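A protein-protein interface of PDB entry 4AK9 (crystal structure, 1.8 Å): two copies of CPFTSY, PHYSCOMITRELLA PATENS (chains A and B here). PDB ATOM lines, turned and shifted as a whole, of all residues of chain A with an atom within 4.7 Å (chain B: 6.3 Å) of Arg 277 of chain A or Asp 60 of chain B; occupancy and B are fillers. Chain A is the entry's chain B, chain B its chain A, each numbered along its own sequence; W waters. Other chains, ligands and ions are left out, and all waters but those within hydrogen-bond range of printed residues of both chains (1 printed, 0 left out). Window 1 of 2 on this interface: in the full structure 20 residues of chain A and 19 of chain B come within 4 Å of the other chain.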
ATOM      1  N   THR A  26     -22.944  -4.088  28.737  1.00  0.00           N
ATOM      2  CA  THR A  26     -21.967  -5.160  28.856  1.00  0.00           C
ATOM      3  C   THR A  26     -21.919  -5.581  30.319  1.00  0.00           C
ATOM      4  O   THR A  26     -21.895  -6.764  30.651  1.00  0.00           O
ATOM      5  CB  THR A  26     -20.555  -4.749  28.373  1.00  0.00           C
ATOM      6  OG1 THR A  26     -20.586  -4.508  26.956  1.00  0.00           O
ATOM      7  CG2 THR A  26     -19.558  -5.890  28.657  1.00  0.00           C
ATOM      8  N   SER A  59     -20.501 -12.016  26.385  1.00  0.00           N
ATOM      9  CA  SER A  59     -20.006 -10.640  26.164  1.00  0.00           C
ATOM     10  C   SER A  59     -18.878 -10.464  25.137  1.00  0.00           C
ATOM     11  O   SER A  59     -18.248  -9.418  25.108  1.00  0.00           O
ATOM     12  CB  SER A  59     -19.556 -10.009  27.499  1.00  0.00           C
ATOM     13  OG  SER A  59     -20.664  -9.865  28.379  1.00  0.00           O
ATOM     14  N   ASP A  60     -18.606 -11.483  24.299  1.00  0.00           N
ATOM     15  CA  ASP A  60     -17.607 -11.332  23.213  1.00  0.00           C
ATOM     16  C   ASP A  60     -16.150 -11.179  23.591  1.00  0.00           C
ATOM     17  O   ASP A  60     -15.346 -10.623  22.859  1.00  0.00           O
ATOM     18  CB  ASP A  60     -18.023 -10.251  22.182  1.00  0.00           C
ATOM     19  CG  ASP A  60     -18.550 -10.865  20.884  1.00  0.00           C
ATOM     20  OD1 ASP A  60     -18.712 -12.110  20.846  1.00  0.00           O
ATOM     21  OD2 ASP A  60     -18.789 -10.110  19.905  1.00  0.00           O
ATOM     22  N   THR A 246     -20.366  -2.255  17.742  1.00  0.00           N
ATOM     23  CA  THR A 246     -21.585  -3.079  17.733  1.00  0.00           C
ATOM     24  C   THR A 246     -21.428  -4.384  16.981  1.00  0.00           C
ATOM     25  O   THR A 246     -22.241  -5.289  17.177  1.00  0.00           O
ATOM     26  CB  THR A 246     -22.837  -2.352  17.216  1.00  0.00           C
ATOM     27  OG1 THR A 246     -22.688  -2.037  15.828  1.00  0.00           O
ATOM     28  CG2 THR A 246     -23.120  -1.123  18.064  1.00  0.00           C
ATOM     29  N   THR A 247     -20.419  -4.486  16.117  1.00  0.00           N
ATOM     30  CA  THR A 247     -20.179  -5.759  15.417  1.00  0.00           C
ATOM     31  C   THR A 247     -19.411  -6.726  16.311  1.00  0.00           C
ATOM     32  O   THR A 247     -19.202  -7.893  15.967  1.00  0.00           O
ATOM     33  CB  THR A 247     -19.452  -5.564  14.076  1.00  0.00           C
ATOM     34  OG1 THR A 247     -18.128  -5.055  14.304  1.00  0.00           O
ATOM     35  CG2 THR A 247     -20.252  -4.613  13.176  1.00  0.00           C
ATOM     36  N   GLY A 248     -18.983  -6.235  17.466  1.00  0.00           N
ATOM     37  CA  GLY A 248     -18.277  -7.096  18.409  1.00  0.00           C
ATOM     38  C   GLY A 248     -17.070  -7.804  17.831  1.00  0.00           C
ATOM     39  O   GLY A 248     -16.252  -7.213  17.125  1.00  0.00           O
ATOM     40  N   LEU A 249     -16.948  -9.098  18.121  1.00  0.00           N
ATOM     41  CA  LEU A 249     -15.769  -9.864  17.709  1.00  0.00           C
ATOM     42  C   LEU A 249     -15.647  -9.937  16.185  1.00  0.00           C
ATOM     43  O   LEU A 249     -14.582 -10.190  15.637  1.00  0.00           O
ATOM     44  CB  LEU A 249     -15.885 -11.291  18.264  1.00  0.00           C
ATOM     45  CG  LEU A 249     -14.538 -11.995  18.452  1.00  0.00           C
ATOM     46  CD1 LEU A 249     -13.857 -11.394  19.668  1.00  0.00           C
ATOM     47  CD2 LEU A 249     -14.722 -13.497  18.646  1.00  0.00           C
ATOM     48  N   ASN A 250     -16.770  -9.769  15.496  1.00  0.00           N
ATOM     49  CA  ASN A 250     -16.730  -9.751  14.039  1.00  0.00           C
ATOM     50  C   ASN A 250     -15.824  -8.675  13.442  1.00  0.00           C
ATOM     51  O   ASN A 250     -15.397  -8.810  12.291  1.00  0.00           O
ATOM     52  CB  ASN A 250     -18.144  -9.672  13.478  1.00  0.00           C
ATOM     53  CG  ASN A 250     -18.919 -10.899  13.806  1.00  0.00           C
ATOM     54  OD1 ASN A 250     -18.386 -12.010  13.687  1.00  0.00           O
ATOM     55  ND2 ASN A 250     -20.153 -10.733  14.279  1.00  0.00           N
ATOM     56  N   THR A 275     -23.668  -1.464  23.875  1.00  0.00           N
ATOM     57  CA  THR A 275     -23.338  -2.766  23.280  1.00  0.00           C
ATOM     58  C   THR A 275     -23.386  -3.742  24.448  1.00  0.00           C
ATOM     59  O   THR A 275     -23.070  -3.355  25.574  1.00  0.00           O
ATOM     60  CB  THR A 275     -21.915  -2.833  22.617  1.00  0.00           C
ATOM     61  OG1 THR A 275     -21.811  -4.044  21.864  1.00  0.00           O
ATOM     62  CG2 THR A 275     -20.817  -2.829  23.661  1.00  0.00           C
ATOM     63  N   ALA A 276     -23.766  -4.999  24.227  1.00  0.00           N
ATOM     64  CA  ALA A 276     -23.486  -5.940  25.298  1.00  0.00           C
ATOM     65  C   ALA A 276     -22.147  -6.629  25.050  1.00  0.00           C
ATOM     66  O   ALA A 276     -21.588  -7.300  25.942  1.00  0.00           O
ATOM     67  CB  ALA A 276     -24.597  -6.940  25.438  1.00  0.00           C
ATOM     68  N   ARG A 277     -21.601  -6.426  23.858  1.00  0.00           N
ATOM     69  CA  ARG A 277     -20.418  -7.161  23.399  1.00  0.00           C
ATOM     70  C   ARG A 277     -19.095  -6.497  23.754  1.00  0.00           C
ATOM     71  O   ARG A 277     -18.122  -6.613  23.003  1.00  0.00           O
ATOM     72  CB  ARG A 277     -20.554  -7.431  21.874  1.00  0.00           C
ATOM     73  CG  ARG A 277     -21.885  -8.114  21.535  1.00  0.00           C
ATOM     74  CD  ARG A 277     -22.182  -8.134  20.016  1.00  0.00           C
ATOM     75  NE  ARG A 277     -21.302  -9.104  19.373  1.00  0.00           N
ATOM     76  CZ  ARG A 277     -21.504  -9.671  18.190  1.00  0.00           C
ATOM     77  NH1 ARG A 277     -22.561  -9.363  17.455  1.00  0.00           N
ATOM     78  NH2 ARG A 277     -20.619 -10.546  17.738  1.00  0.00           N
ATOM     79  N   GLY A 278     -19.032  -5.848  24.923  1.00  0.00           N
ATOM     80  CA  GLY A 278     -17.865  -5.063  25.303  1.00  0.00           C
ATOM     81  C   GLY A 278     -16.562  -5.836  25.491  1.00  0.00           C
ATOM     82  O   GLY A 278     -15.469  -5.251  25.477  1.00  0.00           O
ATOM     83  N   GLY A 279     -16.671  -7.151  25.681  1.00  0.00           N
ATOM     84  CA  GLY A 279     -15.479  -7.995  25.754  1.00  0.00           C
ATOM     85  C   GLY A 279     -14.629  -7.959  24.501  1.00  0.00           C
ATOM     86  O   GLY A 279     -13.440  -8.346  24.528  1.00  0.00           O
ATOM     87  N   CYS A 280     -15.223  -7.506  23.390  1.00  0.00           N
ATOM     88  CA  CYS A 280     -14.476  -7.414  22.124  1.00  0.00           C
ATOM     89  C   CYS A 280     -13.270  -6.498  22.208  1.00  0.00           C
ATOM     90  O   CYS A 280     -12.311  -6.676  21.451  1.00  0.00           O
ATOM     91  CB  CYS A 280     -15.406  -6.994  20.956  1.00  0.00           C
ATOM     92  SG  CYS A 280     -15.941  -5.316  21.031  1.00  0.00           S
ATOM     93  N   VAL B  55     -24.775  -4.465   9.412  1.00  0.00           N
ATOM     94  CA  VAL B  55     -25.963  -4.757  10.183  1.00  0.00           C
ATOM     95  C   VAL B  55     -26.081  -6.274  10.406  1.00  0.00           C
ATOM     96  O   VAL B  55     -26.369  -6.753  11.535  1.00  0.00           O
ATOM     97  CB  VAL B  55     -27.213  -4.171   9.501  1.00  0.00           C
ATOM     98  CG1 VAL B  55     -28.447  -4.739  10.141  1.00  0.00           C
ATOM     99  CG2 VAL B  55     -27.177  -2.628   9.631  1.00  0.00           C
ATOM    100  N   LEU B  56     -25.806  -7.050   9.370  1.00  0.00           N
ATOM    101  CA  LEU B  56     -25.773  -8.507   9.507  1.00  0.00           C
ATOM    102  C   LEU B  56     -24.737  -8.995  10.525  1.00  0.00           C
ATOM    103  O   LEU B  56     -25.034  -9.917  11.301  1.00  0.00           O
ATOM    104  CB  LEU B  56     -25.511  -9.195   8.170  1.00  0.00           C
ATOM    105  CG  LEU B  56     -26.521  -8.903   7.044  1.00  0.00           C
ATOM    106  CD1 LEU B  56     -26.194  -9.768   5.833  1.00  0.00           C
ATOM    107  CD2 LEU B  56     -27.957  -9.138   7.531  1.00  0.00           C
ATOM    108  N   LEU B  57     -23.566  -8.383  10.544  1.00  0.00           N
ATOM    109  CA  LEU B  57     -22.508  -8.755  11.489  1.00  0.00           C
ATOM    110  C   LEU B  57     -22.961  -8.501  12.932  1.00  0.00           C
ATOM    111  O   LEU B  57     -22.643  -9.296  13.840  1.00  0.00           O
ATOM    112  CB  LEU B  57     -21.182  -8.021  11.183  1.00  0.00           C
ATOM    113  CG  LEU B  57     -20.459  -8.358   9.864  1.00  0.00           C
ATOM    114  CD1 LEU B  57     -19.185  -7.494   9.728  1.00  0.00           C
ATOM    115  CD2 LEU B  57     -20.071  -9.830   9.742  1.00  0.00           C
ATOM    116  N   VAL B  58     -23.727  -7.448  13.146  1.00  0.00           N
ATOM    117  CA  VAL B  58     -24.260  -7.157  14.467  1.00  0.00           C
ATOM    118  C   VAL B  58     -25.132  -8.323  14.962  1.00  0.00           C
ATOM    119  O   VAL B  58     -25.095  -8.693  16.141  1.00  0.00           O
ATOM    120  CB  VAL B  58     -25.010  -5.804  14.487  1.00  0.00           C
ATOM    121  CG1 VAL B  58     -25.663  -5.571  15.860  1.00  0.00           C
ATOM    122  CG2 VAL B  58     -24.044  -4.651  14.111  1.00  0.00           C
ATOM    123  N   SER B  59     -25.910  -8.930  14.071  1.00  0.00           N
ATOM    124  CA  SER B  59     -26.709 -10.093  14.431  1.00  0.00           C
ATOM    125  C   SER B  59     -25.969 -11.438  14.314  1.00  0.00           C
ATOM    126  O   SER B  59     -26.583 -12.500  14.389  1.00  0.00           O
ATOM    127  CB  SER B  59     -28.032 -10.136  13.650  1.00  0.00           C
ATOM    128  OG  SER B  59     -28.905  -9.099  14.097  1.00  0.00           O
ATOM    129  N   ASP B  60     -24.648 -11.419  14.180  1.00  0.00           N
ATOM    130  CA  ASP B  60     -23.880 -12.670  14.091  1.00  0.00           C
ATOM    131  C   ASP B  60     -24.123 -13.592  12.902  1.00  0.00           C
ATOM    132  O   ASP B  60     -23.934 -14.806  12.992  1.00  0.00           O
ATOM    133  CB  ASP B  60     -23.957 -13.466  15.396  1.00  0.00           C
ATOM    134  CG  ASP B  60     -22.767 -13.176  16.295  1.00  0.00           C
ATOM    135  OD1 ASP B  60     -21.941 -12.297  15.933  1.00  0.00           O
ATOM    136  OD2 ASP B  60     -22.645 -13.831  17.351  1.00  0.00           O
ATOM    137  N   PHE B  61     -24.555 -13.027  11.779  1.00  0.00           N
ATOM    138  CA  PHE B  61     -24.087 -13.560  10.508  1.00  0.00           C
ATOM    139  C   PHE B  61     -22.570 -13.303  10.508  1.00  0.00           C
ATOM    140  O   PHE B  61     -22.125 -12.142  10.583  1.00  0.00           O
ATOM    141  CB  PHE B  61     -24.746 -12.808   9.356  1.00  0.00           C
ATOM    142  CG  PHE B  61     -26.229 -12.984   9.285  1.00  0.00           C
ATOM    143  CD1 PHE B  61     -27.078 -12.220  10.085  1.00  0.00           C
ATOM    144  CD2 PHE B  61     -26.782 -13.880   8.387  1.00  0.00           C
ATOM    145  CE1 PHE B  61     -28.439 -12.359  10.015  1.00  0.00           C
ATOM    146  CE2 PHE B  61     -28.160 -14.028   8.311  1.00  0.00           C
ATOM    147  CZ  PHE B  61     -28.992 -13.266   9.116  1.00  0.00           C
ATOM    148  N   GLY B  62     -21.765 -14.369  10.489  1.00  0.00           N
ATOM    149  CA  GLY B  62     -20.319 -14.192  10.614  1.00  0.00           C
ATOM    150  C   GLY B  62     -19.685 -13.553   9.374  1.00  0.00           C
ATOM    151  O   GLY B  62     -20.331 -13.478   8.317  1.00  0.00           O
ATOM    152  N   THR B 247     -24.373 -17.456  23.078  1.00  0.00           N
ATOM    153  CA  THR B 247     -22.966 -17.272  22.761  1.00  0.00           C
ATOM    154  C   THR B 247     -22.777 -16.897  21.306  1.00  0.00           C
ATOM    155  O   THR B 247     -21.672 -16.576  20.887  1.00  0.00           O
ATOM    156  CB  THR B 247     -22.107 -18.522  23.121  1.00  0.00           C
ATOM    157  OG1 THR B 247     -22.476 -19.632  22.285  1.00  0.00           O
ATOM    158  CG2 THR B 247     -22.325 -18.863  24.579  1.00  0.00           C
ATOM    159  N   GLY B 248     -23.866 -16.923  20.544  1.00  0.00           N
ATOM    160  CA  GLY B 248     -23.805 -16.516  19.141  1.00  0.00           C
ATOM    161  C   GLY B 248     -22.756 -17.250  18.328  1.00  0.00           C
ATOM    162  O   GLY B 248     -22.585 -18.474  18.429  1.00  0.00           O
ATOM    163  N   LEU B 249     -22.001 -16.497  17.534  1.00  0.00           N
ATOM    164  CA  LEU B 249     -21.042 -17.098  16.615  1.00  0.00           C
ATOM    165  C   LEU B 249     -19.943 -17.822  17.382  1.00  0.00           C
ATOM    166  O   LEU B 249     -19.236 -18.690  16.856  1.00  0.00           O
ATOM    167  CB  LEU B 249     -20.422 -16.003  15.743  1.00  0.00           C
ATOM    168  CG  LEU B 249     -19.861 -16.446  14.396  1.00  0.00           C
ATOM    169  CD1 LEU B 249     -21.003 -16.720  13.442  1.00  0.00           C
ATOM    170  CD2 LEU B 249     -18.952 -15.374  13.824  1.00  0.00           C
ATOM    171  N   ASN B 250     -19.774 -17.435  18.641  1.00  0.00           N
ATOM    172  CA  ASN B 250     -18.780 -18.111  19.464  1.00  0.00           C
ATOM    173  C   ASN B 250     -19.027 -19.596  19.638  1.00  0.00           C
ATOM    174  O   ASN B 250     -18.095 -20.331  19.978  1.00  0.00           O
ATOM    175  CB  ASN B 250     -18.626 -17.384  20.817  1.00  0.00           C
ATOM    176  CG  ASN B 250     -18.008 -16.028  20.649  1.00  0.00           C
ATOM    177  OD1 ASN B 250     -17.102 -15.825  19.802  1.00  0.00           O
ATOM    178  ND2 ASN B 250     -18.505 -15.064  21.422  1.00  0.00           N
ATOM    179  N   ALA B 276     -29.821 -11.057  20.520  1.00  0.00           N
ATOM    180  CA  ALA B 276     -29.997 -10.386  19.226  1.00  0.00           C
ATOM    181  C   ALA B 276     -29.162 -11.078  18.149  1.00  0.00           C
ATOM    182  O   ALA B 276     -29.171 -10.686  16.973  1.00  0.00           O
ATOM    183  CB  ALA B 276     -29.567  -8.921  19.362  1.00  0.00           C
ATOM    184  N   ARG B 277     -28.442 -12.130  18.539  1.00  0.00           N
ATOM    185  CA  ARG B 277     -27.442 -12.747  17.666  1.00  0.00           C
ATOM    186  C   ARG B 277     -28.000 -13.941  16.902  1.00  0.00           C
ATOM    187  O   ARG B 277     -27.271 -14.903  16.647  1.00  0.00           O
ATOM    188  CB  ARG B 277     -26.175 -13.130  18.495  1.00  0.00           C
ATOM    189  CG  ARG B 277     -25.592 -11.917  19.235  1.00  0.00           C
ATOM    190  CD  ARG B 277     -24.633 -12.308  20.388  1.00  0.00           C
ATOM    191  NE  ARG B 277     -23.382 -12.755  19.811  1.00  0.00           N
ATOM    192  CZ  ARG B 277     -22.249 -12.953  20.474  1.00  0.00           C
ATOM    193  NH1 ARG B 277     -22.185 -12.742  21.778  1.00  0.00           N
ATOM    194  NH2 ARG B 277     -21.179 -13.357  19.801  1.00  0.00           N
ATOM    195  N   GLY B 278     -29.276 -13.863  16.509  1.00  0.00           N
ATOM    196  CA  GLY B 278     -29.957 -14.949  15.810  1.00  0.00           C
ATOM    197  C   GLY B 278     -29.396 -15.364  14.445  1.00  0.00           C
ATOM    198  O   GLY B 278     -29.693 -16.476  13.965  1.00  0.00           O
ATOM    199  N   GLY B 279     -28.565 -14.510  13.845  1.00  0.00           N
ATOM    200  CA  GLY B 279     -27.878 -14.826  12.593  1.00  0.00           C
ATOM    201  C   GLY B 279     -26.939 -16.012  12.763  1.00  0.00           C
ATOM    202  O   GLY B 279     -26.523 -16.638  11.780  1.00  0.00           O
ATOM    203  N   CYS B 280     -26.605 -16.352  14.017  1.00  0.00           N
ATOM    204  CA  CYS B 280     -25.721 -17.490  14.266  1.00  0.00           C
ATOM    205  C   CYS B 280     -26.302 -18.800  13.708  1.00  0.00           C
ATOM    206  O   CYS B 280     -25.553 -19.705  13.319  1.00  0.00           O
ATOM    207  CB  CYS B 280     -25.380 -17.646  15.766  1.00  0.00           C
ATOM    208  SG  CYS B 280     -26.755 -18.182  16.805  1.00  0.00           S
ATOM    209  N   VAL B 281     -27.624 -18.889  13.633  1.00  0.00           N
ATOM    210  CA  VAL B 281     -28.280 -20.023  12.976  1.00  0.00           C
ATOM    211  C   VAL B 281     -27.788 -20.190  11.527  1.00  0.00           C
ATOM    212  O   VAL B 281     -27.507 -21.316  11.064  1.00  0.00           O
ATOM    213  CB  VAL B 281     -29.805 -19.849  12.996  1.00  0.00           C
ATOM    214  CG1 VAL B 281     -30.507 -20.947  12.183  1.00  0.00           C
ATOM    215  CG2 VAL B 281     -30.303 -19.843  14.437  1.00  0.00           C
ATOM    216  N   VAL B 282     -27.731 -19.090  10.793  1.00  0.00           N
ATOM    217  CA  VAL B 282     -27.308 -19.139   9.401  1.00  0.00           C
ATOM    218  C   VAL B 282     -25.832 -19.463   9.296  1.00  0.00           C
ATOM    219  O   VAL B 282     -25.412 -20.305   8.502  1.00  0.00           O
ATOM    220  CB  VAL B 282     -27.626 -17.782   8.701  1.00  0.00           C
ATOM    221  CG1 VAL B 282     -27.254 -17.861   7.194  1.00  0.00           C
ATOM    222  CG2 VAL B 282     -29.092 -17.459   8.900  1.00  0.00           C
ATOM    223  N   SER B 283     -25.041 -18.830  10.141  1.00  0.00           N
ATOM    224  CA  SER B 283     -23.599 -19.035  10.120  1.00  0.00           C
ATOM    225  C   SER B 283     -23.213 -20.471  10.409  1.00  0.00           C
ATOM    226  O   SER B 283     -22.295 -21.012   9.781  1.00  0.00           O
ATOM    227  CB  SER B 283     -22.938 -18.126  11.143  1.00  0.00           C
ATOM    228  OG  SER B 283     -23.222 -16.747  10.828  1.00  0.00           O
HETATM  229  O   HOH W   1     -19.014 -13.177  17.540  1.00  0.00           O
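Ser 59 of chain A touches none of the printed residues of chain B. Of the printed residues of chain B, Thr 247 of chain A touches Val 58. Of the printed residues of chain B, Leu 249 of chain A touches Asn 250 (3.5 Å). Of chain B, only Leu 57, Val 58, Asp 60 and Arg 277 come within 4 Å of Arg 277 of chain A. Gly 279 of chain A touches none of the printed residues of chain B. Of the printed residues of chain A, Leu 249 of chain B touches Asn 250. Of the printed residues of chain A, Arg 277 of chain B touches Asp 60 and Arg 277. The nearest residue of chain B that does not touch Arg 277 of chain A is Ser 59 of chain B (4.8 Å). The nearest printed residue of chain B that does not touch Leu 249 of chain A is Arg 277 of chain B (5.9 Å).
O of Leu 57 of chain B lies within hydrogen-bond range of ND2 of Asn 250 of chain A, 2.9 Å away. The side-chain carboxylate (OD1) of Asp 60 of chain B lies within salt-bridge range of the guanidinium group (NH2) of Arg 277 of chain A (2.8 Å). The side-chain carboxylate (OD1) of Asp 60 of chain A lies within salt-bridge range of the guanidinium group (NH2) of Arg 277 of chain B, at 3.0 Å. OD1 of Asp 60 of chain A is in hydrogen-bond range of ND2 of Asn 250 of chain B (3.0 Å). NH1 of Arg 277 of chain A is in hydrogen-bond range of O of Val 58 of chain B (2.9 Å). The side-chain carboxylate of Asp 60 of chain B lies within hydrogen-bond range of the side-chain amide nitrogen of Asn 250 of chain A, 2.9 Å away.
Of the 14 printed residues of chain A, 6 touch a printed residue of chain B. Printed residues of chain A that touch a printed residue of chain B: Asp 60, Thr 246, Thr 247, Leu 249, Asn 250 and Arg 277. Of the 20 printed residues of chain B, 6 touch a printed residue of chain A.
Asp 60 of chain A touches Asn 250 of chain B, and with the chains exchanged Asn 250 of chain A touches Asp 60 of chain B. Asp 60 of chain A touches Arg 277 of chain B, and with the chains exchanged Arg 277 of chain A touches Asp 60 of chain B. Leu 249 of chain A touches Asn 250 of chain B, and with the chains exchanged Asn 250 of chain A touches Leu 249 of chain B. Arg 277 of chain B touches its own counterpart, Arg 277 of chain A. Of the 12 pairs that touch across the chains among the printed residues, 7 have their exchanged pair printed and touching as well.
Water W1 lies within hydrogen-bond range of the guanidinium group of Arg 277 of chain A, the guanidinium group of Arg 277 of chain B, the side-chain carboxylate of Asp 60 of chain B and the side-chain carboxylate of Asp 60 of chain A.
CG2 of Val 58 of chain B touches OG1 of Thr 246 of chain A, at 3.4 Å. Thr 247 of chain A touches Val 58 of chain B (CG2 to CG2, 3.9 Å). Leu 249 of chain A touches Asn 250 of chain B. OD1 of Asn 250 of chain A touches CD2 of Leu 249 of chain B, at 3.4 Å. Arg 277 of chain A touches Leu 57 of chain B. Arg 277 of chain B touches Arg 277 of chain A (NH2 to NH2, 3.5 Å).
The guanidinium group (NE) of Arg 277 of chain B is in salt-bridge range of the side-chain carboxylate (OD2) of Asp 60 of chain B (2.8 Å). The side-chain hydroxyl (OG) of Ser 283 of chain B is in hydrogen-bond range of the backbone carbonyl oxygen (O) of Asp 60 of chain B (3.0 Å). N of Leu 249 of chain B sits at hydrogen-bond distance from OD2 of Asp 60 of chain B (2.7 Å). The backbone carbonyl oxygen of Thr 247 of chain A lies within hydrogen-bond range of the guanidinium group of Arg 277 of chain A, 3.5 Å away. The backbone carbonyl oxygen (O) of Thr 247 of chain A lies close to the side-chain amide nitrogen (ND2) of Asn 250 of chain A (3.4 Å). O of Arg 277 of chain A is in hydrogen-bond range of SG of Cys 280 of chain A.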
